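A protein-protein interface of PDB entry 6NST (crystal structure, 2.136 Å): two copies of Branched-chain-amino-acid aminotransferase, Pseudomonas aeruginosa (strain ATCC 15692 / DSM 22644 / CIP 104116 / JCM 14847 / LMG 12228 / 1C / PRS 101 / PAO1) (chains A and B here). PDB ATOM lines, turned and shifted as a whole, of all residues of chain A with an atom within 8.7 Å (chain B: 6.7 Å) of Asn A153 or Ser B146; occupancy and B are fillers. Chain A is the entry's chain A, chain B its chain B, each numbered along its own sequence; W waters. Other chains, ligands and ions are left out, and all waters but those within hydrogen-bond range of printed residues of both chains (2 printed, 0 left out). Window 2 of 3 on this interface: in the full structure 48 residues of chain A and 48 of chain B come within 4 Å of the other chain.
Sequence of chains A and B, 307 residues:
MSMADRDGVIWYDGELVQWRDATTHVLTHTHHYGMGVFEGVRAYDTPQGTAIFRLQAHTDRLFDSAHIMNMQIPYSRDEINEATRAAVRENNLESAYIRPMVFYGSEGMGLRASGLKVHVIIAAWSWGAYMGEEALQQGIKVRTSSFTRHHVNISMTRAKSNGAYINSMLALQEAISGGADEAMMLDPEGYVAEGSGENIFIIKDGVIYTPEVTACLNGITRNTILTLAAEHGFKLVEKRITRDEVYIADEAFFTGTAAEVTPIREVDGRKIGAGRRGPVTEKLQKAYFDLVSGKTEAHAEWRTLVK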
ATOM      1  N   HIS A 150      30.296 -24.420  -0.049  1.00  0.00           N
ATOM      2  CA  HIS A 150      29.837 -25.260   1.050  1.00  0.00           C
ATOM      3  C   HIS A 150      29.762 -24.484   2.363  1.00  0.00           C
ATOM      4  O   HIS A 150      30.545 -23.566   2.620  1.00  0.00           O
ATOM      5  CB  HIS A 150      30.763 -26.465   1.216  1.00  0.00           C
ATOM      6  CG  HIS A 150      30.567 -27.526   0.180  1.00  0.00           C
ATOM      7  ND1 HIS A 150      29.428 -28.300   0.115  1.00  0.00           N
ATOM      8  CD2 HIS A 150      31.366 -27.949  -0.828  1.00  0.00           C
ATOM      9  CE1 HIS A 150      29.531 -29.149  -0.891  1.00  0.00           C
ATOM     10  NE2 HIS A 150      30.699 -28.958  -1.479  1.00  0.00           N
ATOM     11  N   HIS A 151      28.805 -24.880   3.200  1.00  0.00           N
ATOM     12  CA  HIS A 151      28.563 -24.273   4.502  1.00  0.00           C
ATOM     13  C   HIS A 151      29.272 -25.090   5.576  1.00  0.00           C
ATOM     14  O   HIS A 151      29.153 -26.319   5.603  1.00  0.00           O
ATOM     15  CB  HIS A 151      27.059 -24.205   4.773  1.00  0.00           C
ATOM     16  CG  HIS A 151      26.688 -23.475   6.026  1.00  0.00           C
ATOM     17  ND1 HIS A 151      26.805 -24.038   7.279  1.00  0.00           N
ATOM     18  CD2 HIS A 151      26.171 -22.239   6.216  1.00  0.00           C
ATOM     19  CE1 HIS A 151      26.393 -23.172   8.188  1.00  0.00           C
ATOM     20  NE2 HIS A 151      26.002 -22.074   7.570  1.00  0.00           N
ATOM     21  N   VAL A 152      29.995 -24.402   6.466  1.00  0.00           N
ATOM     22  CA  VAL A 152      30.886 -25.074   7.411  1.00  0.00           C
ATOM     23  C   VAL A 152      30.152 -26.002   8.367  1.00  0.00           C
ATOM     24  O   VAL A 152      30.786 -26.850   9.004  1.00  0.00           O
ATOM     25  CB  VAL A 152      31.703 -24.040   8.213  1.00  0.00           C
ATOM     26  CG1 VAL A 152      32.614 -23.255   7.291  1.00  0.00           C
ATOM     27  CG2 VAL A 152      30.773 -23.115   8.985  1.00  0.00           C
ATOM     28  N   ASN A 153      28.835 -25.861   8.508  1.00  0.00           N
ATOM     29  CA  ASN A 153      28.065 -26.748   9.367  1.00  0.00           C
ATOM     30  C   ASN A 153      27.111 -27.646   8.592  1.00  0.00           C
ATOM     31  O   ASN A 153      26.324 -28.373   9.208  1.00  0.00           O
ATOM     32  CB  ASN A 153      27.286 -25.944  10.414  1.00  0.00           C
ATOM     33  CG  ASN A 153      26.828 -26.804  11.575  1.00  0.00           C
ATOM     34  OD1 ASN A 153      27.437 -27.830  11.871  1.00  0.00           O
ATOM     35  ND2 ASN A 153      25.741 -26.401  12.224  1.00  0.00           N
ATOM     36  N   ILE A 154      27.150 -27.611   7.266  1.00  0.00           N
ATOM     37  CA  ILE A 154      26.391 -28.539   6.437  1.00  0.00           C
ATOM     38  C   ILE A 154      27.279 -29.652   5.907  1.00  0.00           C
ATOM     39  O   ILE A 154      26.942 -30.832   6.007  1.00  0.00           O
ATOM     40  CB  ILE A 154      25.689 -27.783   5.288  1.00  0.00           C
ATOM     41  CG1 ILE A 154      24.686 -26.777   5.856  1.00  0.00           C
ATOM     42  CG2 ILE A 154      25.009 -28.767   4.351  1.00  0.00           C
ATOM     43  CD1 ILE A 154      23.958 -25.967   4.799  1.00  0.00           C
ATOM     44  N   SER A 155      28.425 -29.294   5.342  1.00  0.00           N
ATOM     45  CA  SER A 155      29.432 -30.261   4.946  1.00  0.00           C
ATOM     46  C   SER A 155      30.729 -29.957   5.681  1.00  0.00           C
ATOM     47  O   SER A 155      30.968 -28.826   6.115  1.00  0.00           O
ATOM     48  CB  SER A 155      29.661 -30.253   3.429  1.00  0.00           C
ATOM     49  OG  SER A 155      30.076 -28.980   2.980  1.00  0.00           O
ATOM     50  N   MET A 156      31.557 -30.984   5.829  1.00  0.00           N
ATOM     51  CA  MET A 156      32.796 -30.878   6.592  1.00  0.00           C
ATOM     52  C   MET A 156      33.877 -30.330   5.671  1.00  0.00           C
ATOM     53  O   MET A 156      34.520 -31.077   4.929  1.00  0.00           O
ATOM     54  CB  MET A 156      33.161 -32.233   7.182  1.00  0.00           C
ATOM     55  CG  MET A 156      32.071 -32.816   8.086  1.00  0.00           C
ATOM     56  SD  MET A 156      31.716 -31.805   9.550  1.00  0.00           S
ATOM     57  CE  MET A 156      30.243 -30.913   9.044  1.00  0.00           C
ATOM     58  N   THR A 157      34.080 -29.009   5.725  1.00  0.00           N
ATOM     59  CA  THR A 157      34.909 -28.313   4.750  1.00  0.00           C
ATOM     60  C   THR A 157      36.396 -28.614   4.895  1.00  0.00           C
ATOM     61  O   THR A 157      37.161 -28.292   3.978  1.00  0.00           O
ATOM     62  CB  THR A 157      34.674 -26.802   4.850  1.00  0.00           C
ATOM     63  OG1 THR A 157      34.953 -26.354   6.182  1.00  0.00           O
ATOM     64  CG2 THR A 157      33.228 -26.464   4.500  1.00  0.00           C
ATOM     65  N   PRO A 188      28.611 -18.779   2.160  1.00  0.00           N
ATOM     66  CA  PRO A 188      27.231 -18.349   2.463  1.00  0.00           C
ATOM     67  C   PRO A 188      27.101 -16.914   2.964  1.00  0.00           C
ATOM     68  O   PRO A 188      25.976 -16.402   3.018  1.00  0.00           O
ATOM     69  CB  PRO A 188      26.783 -19.352   3.534  1.00  0.00           C
ATOM     70  CG  PRO A 188      27.546 -20.585   3.205  1.00  0.00           C
ATOM     71  CD  PRO A 188      28.896 -20.109   2.732  1.00  0.00           C
ATOM     72  N   THR A 214      38.660 -20.504   6.316  1.00  0.00           N
ATOM     73  CA  THR A 214      37.359 -20.334   6.947  1.00  0.00           C
ATOM     74  C   THR A 214      36.382 -21.386   6.442  1.00  0.00           C
ATOM     75  O   THR A 214      36.168 -22.412   7.096  1.00  0.00           O
ATOM     76  CB  THR A 214      36.823 -18.927   6.672  1.00  0.00           C
ATOM     77  OG1 THR A 214      37.922 -18.014   6.558  1.00  0.00           O
ATOM     78  CG2 THR A 214      35.932 -18.469   7.801  1.00  0.00           C
ATOM     79  N   ALA A 215      35.788 -21.142   5.277  1.00  0.00           N
ATOM     80  CA  ALA A 215      34.895 -22.098   4.640  1.00  0.00           C
ATOM     81  C   ALA A 215      35.506 -22.742   3.403  1.00  0.00           C
ATOM     82  O   ALA A 215      34.860 -23.591   2.778  1.00  0.00           O
ATOM     83  CB  ALA A 215      33.570 -21.420   4.277  1.00  0.00           C
ATOM     84  N   ARG B 143      16.515 -37.213  17.883  1.00  0.00           N
ATOM     85  CA  ARG B 143      17.354 -36.149  18.413  1.00  0.00           C
ATOM     86  C   ARG B 143      17.675 -35.172  17.293  1.00  0.00           C
ATOM     87  O   ARG B 143      18.115 -35.583  16.215  1.00  0.00           O
ATOM     88  CB  ARG B 143      18.647 -36.706  19.022  1.00  0.00           C
ATOM     89  CG  ARG B 143      18.481 -37.279  20.423  1.00  0.00           C
ATOM     90  CD  ARG B 143      19.771 -37.913  20.923  1.00  0.00           C
ATOM     91  NE  ARG B 143      20.801 -36.918  21.202  1.00  0.00           N
ATOM     92  CZ  ARG B 143      20.959 -36.321  22.379  1.00  0.00           C
ATOM     93  NH1 ARG B 143      20.150 -36.619  23.386  1.00  0.00           N
ATOM     94  NH2 ARG B 143      21.923 -35.425  22.547  1.00  0.00           N
ATOM     95  N   THR B 144      17.440 -33.886  17.547  1.00  0.00           N
ATOM     96  CA  THR B 144      17.755 -32.859  16.564  1.00  0.00           C
ATOM     97  C   THR B 144      19.234 -32.910  16.209  1.00  0.00           C
ATOM     98  O   THR B 144      20.092 -33.062  17.084  1.00  0.00           O
ATOM     99  CB  THR B 144      17.385 -31.479  17.111  1.00  0.00           C
ATOM    100  OG1 THR B 144      15.995 -31.466  17.459  1.00  0.00           O
ATOM    101  CG2 THR B 144      17.650 -30.402  16.074  1.00  0.00           C
ATOM    102  N   SER B 145      19.531 -32.802  14.916  1.00  0.00           N
ATOM    103  CA  SER B 145      20.904 -32.886  14.445  1.00  0.00           C
ATOM    104  C   SER B 145      21.629 -31.561  14.638  1.00  0.00           C
ATOM    105  O   SER B 145      21.085 -30.489  14.358  1.00  0.00           O
ATOM    106  CB  SER B 145      20.938 -33.283  12.969  1.00  0.00           C
ATOM    107  OG  SER B 145      22.253 -33.178  12.446  1.00  0.00           O
ATOM    108  N   SER B 146      22.868 -31.640  15.128  1.00  0.00           N
ATOM    109  CA  SER B 146      23.717 -30.456  15.168  1.00  0.00           C
ATOM    110  C   SER B 146      24.227 -30.088  13.783  1.00  0.00           C
ATOM    111  O   SER B 146      24.686 -28.959  13.583  1.00  0.00           O
ATOM    112  CB  SER B 146      24.895 -30.674  16.119  1.00  0.00           C
ATOM    113  OG  SER B 146      25.797 -31.639  15.595  1.00  0.00           O
ATOM    114  N   PHE B 147      24.162 -31.014  12.830  1.00  0.00           N
ATOM    115  CA  PHE B 147      24.491 -30.709  11.446  1.00  0.00           C
ATOM    116  C   PHE B 147      23.293 -30.058  10.771  1.00  0.00           C
ATOM    117  O   PHE B 147      22.166 -30.554  10.871  1.00  0.00           O
ATOM    118  CB  PHE B 147      24.896 -31.976  10.695  1.00  0.00           C
ATOM    119  CG  PHE B 147      26.087 -32.672  11.281  1.00  0.00           C
ATOM    120  CD1 PHE B 147      27.371 -32.244  10.985  1.00  0.00           C
ATOM    121  CD2 PHE B 147      25.924 -33.759  12.122  1.00  0.00           C
ATOM    122  CE1 PHE B 147      28.473 -32.886  11.523  1.00  0.00           C
ATOM    123  CE2 PHE B 147      27.019 -34.406  12.663  1.00  0.00           C
ATOM    124  CZ  PHE B 147      28.297 -33.968  12.363  1.00  0.00           C
ATOM    125  N   THR B 148      23.540 -28.945  10.090  1.00  0.00           N
ATOM    126  CA  THR B 148      22.484 -28.221   9.399  1.00  0.00           C
ATOM    127  C   THR B 148      22.122 -28.927   8.098  1.00  0.00           C
ATOM    128  O   THR B 148      22.993 -29.451   7.397  1.00  0.00           O
ATOM    129  CB  THR B 148      22.932 -26.785   9.119  1.00  0.00           C
ATOM    130  OG1 THR B 148      23.261 -26.140  10.356  1.00  0.00           O
ATOM    131  CG2 THR B 148      21.836 -26.000   8.423  1.00  0.00           C
ATOM    132  N   ARG B 149      20.828 -28.947   7.783  1.00  0.00           N
ATOM    133  CA  ARG B 149      20.358 -29.539   6.540  1.00  0.00           C
ATOM    134  C   ARG B 149      20.860 -28.728   5.344  1.00  0.00           C
ATOM    135  O   ARG B 149      21.327 -27.594   5.478  1.00  0.00           O
ATOM    136  CB  ARG B 149      18.830 -29.626   6.534  1.00  0.00           C
ATOM    137  CG  ARG B 149      18.260 -30.644   5.557  1.00  0.00           C
ATOM    138  CD  ARG B 149      18.980 -31.979   5.688  1.00  0.00           C
ATOM    139  NE  ARG B 149      18.400 -33.011   4.833  1.00  0.00           N
ATOM    140  CZ  ARG B 149      18.874 -34.249   4.734  1.00  0.00           C
ATOM    141  NH1 ARG B 149      19.939 -34.611   5.436  1.00  0.00           N
ATOM    142  NH2 ARG B 149      18.284 -35.125   3.932  1.00  0.00           N
ATOM    143  N   ASN B 167      25.492 -35.667   4.336  1.00  0.00           N
ATOM    144  CA  ASN B 167      24.891 -34.908   5.426  1.00  0.00           C
ATOM    145  C   ASN B 167      23.891 -35.757   6.203  1.00  0.00           C
ATOM    146  O   ASN B 167      23.829 -35.684   7.436  1.00  0.00           O
ATOM    147  CB  ASN B 167      24.233 -33.650   4.856  1.00  0.00           C
ATOM    148  CG  ASN B 167      23.461 -32.866   5.890  1.00  0.00           C
ATOM    149  OD1 ASN B 167      22.252 -33.038   6.034  1.00  0.00           O
ATOM    150  ND2 ASN B 167      24.151 -31.986   6.606  1.00  0.00           N
ATOM    151  N   ALA B 171      24.297 -37.052  10.301  1.00  0.00           N
ATOM    152  CA  ALA B 171      23.259 -36.770  11.286  1.00  0.00           C
ATOM    153  C   ALA B 171      22.680 -38.049  11.875  1.00  0.00           C
ATOM    154  O   ALA B 171      22.370 -38.096  13.070  1.00  0.00           O
ATOM    155  CB  ALA B 171      22.153 -35.927  10.655  1.00  0.00           C
ATOM    156  N   GLU B 174      25.140 -39.339  14.386  1.00  0.00           N
ATOM    157  CA  GLU B 174      25.094 -38.529  15.598  1.00  0.00           C
ATOM    158  C   GLU B 174      23.909 -38.916  16.472  1.00  0.00           C
ATOM    159  O   GLU B 174      24.057 -39.123  17.683  1.00  0.00           O
ATOM    160  CB  GLU B 174      25.026 -37.045  15.236  1.00  0.00           C
ATOM    161  CG  GLU B 174      24.846 -36.129  16.438  1.00  0.00           C
ATOM    162  CD  GLU B 174      24.619 -34.678  16.051  1.00  0.00           C
ATOM    163  OE1 GLU B 174      23.730 -34.411  15.218  1.00  0.00           O
ATOM    164  OE2 GLU B 174      25.331 -33.804  16.582  1.00  0.00           O
ATOM    165  N   MET B 184      16.457 -35.208  13.519  1.00  0.00           N
ATOM    166  CA  MET B 184      15.585 -34.186  12.952  1.00  0.00           C
ATOM    167  C   MET B 184      16.458 -33.062  12.408  1.00  0.00           C
ATOM    168  O   MET B 184      17.234 -32.460  13.157  1.00  0.00           O
ATOM    169  CB  MET B 184      14.596 -33.652  13.990  1.00  0.00           C
ATOM    170  CG  MET B 184      13.519 -32.752  13.397  1.00  0.00           C
ATOM    171  SD  MET B 184      12.254 -32.253  14.579  1.00  0.00           S
ATOM    172  CE  MET B 184      13.223 -31.301  15.743  1.00  0.00           C
HETATM  173  O   HOH W   1      24.694 -23.757  10.872  1.00  0.00           O
HETATM  174  O   HOH W   2      27.808 -33.113   4.516  1.00  0.00           O
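The side-chain amide nitrogen of Asn A153 lies within hydrogen-bond range of the backbone carbonyl oxygen of Ser B146.
O of Asn A153 sits at hydrogen-bond distance from N of Thr B148, at 3.0 Å.
ND2 of Asn B167 sits at hydrogen-bond distance from O of Ile A154, 3.1 Å away.
Of the printed residues of chain A, Ser B146 touches Asn A153 (3.1 Å).
No residue of chain A comes within 4 Å of Ser B145.
Of the printed residues of chain B, Met A156 touches Phe B147.
Of the printed residues of chain A, Phe B147 touches Asn A153 (3.7 Å) and Met A156 (3.6 Å).
Of the printed residues of chain A, Thr B148 touches Asn A153 (3.0 Å) and Ile A154 (3.5 Å).
Of the printed residues of chain A, Asn B167 touches Ile A154.
Met B184 touches none of the printed residues of chain A.
The nearest residue of chain B that does not touch Asn A153 is Asn B167 (5.0 Å).
The nearest printed residue of chain A that does not touch Arg B149 is Asn A153 (5.7 Å).
Printed residues of chain A that touch a printed residue of chain B: Asn A153, Ile A154 and Met A156.
Hydrophobic or aromatic side chains of chain A within 4 Å of the printed part of chain B: Ile A154 and Met A156.
Of the 11 printed residues of chain B, 5 touch a printed residue of chain A.
Hydrophobic or aromatic side chains of chain B within 4 Å of the printed part of chain A: Phe B147.
Along chain B the printed residues that touch a printed residue of chain A span positions 146 to 167.
Among the printed residues, no Asp or Glu carboxylate lies within 4 Å of a Lys or Arg side-chain nitrogen of the other chain.
No position is printed for both chains.
Of the 7 pairs that touch across the chains among the printed residues, none has its exchanged pair printed and touching as well.
A ring nitrogen (ND1) of His A151 lies within hydrogen-bond range of the backbone NH (N) of Asn A153.
The side-chain hydroxyl (OG) of Ser B145 sits at hydrogen-bond distance from the backbone NH (N) of Phe B147 (2.9 Å).
The side-chain carboxylate of Glu B174 is in hydrogen-bond range of the side-chain hydroxyl of Ser B146.
The backbone carbonyl oxygen (O) of Thr B148 lies within hydrogen-bond range of the side-chain amide nitrogen (ND2) of Asn B167.
The guanidinium group (NH1) of Arg B149 is in hydrogen-bond range of the side-chain amide oxygen (OD1) of Asn B167.
Phe B147 touches Asn A153.
Ile A154 touches Thr B148 (CG1 to O, 3.5 Å).
CD1 of Ile A154 touches O of Arg B149, at 3.2 Å.
Met A156 touches Phe B147.
Water W1 bridges the side-chain hydroxyl (OG1) of Thr B148 (2.8 Å) and the side-chain amide nitrogen (ND2) of Asn A153 (3.1 Å).
Water W2 bridges the backbone carbonyl oxygen (O) of Ile A154 and the backbone NH (N) of Asn B167.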
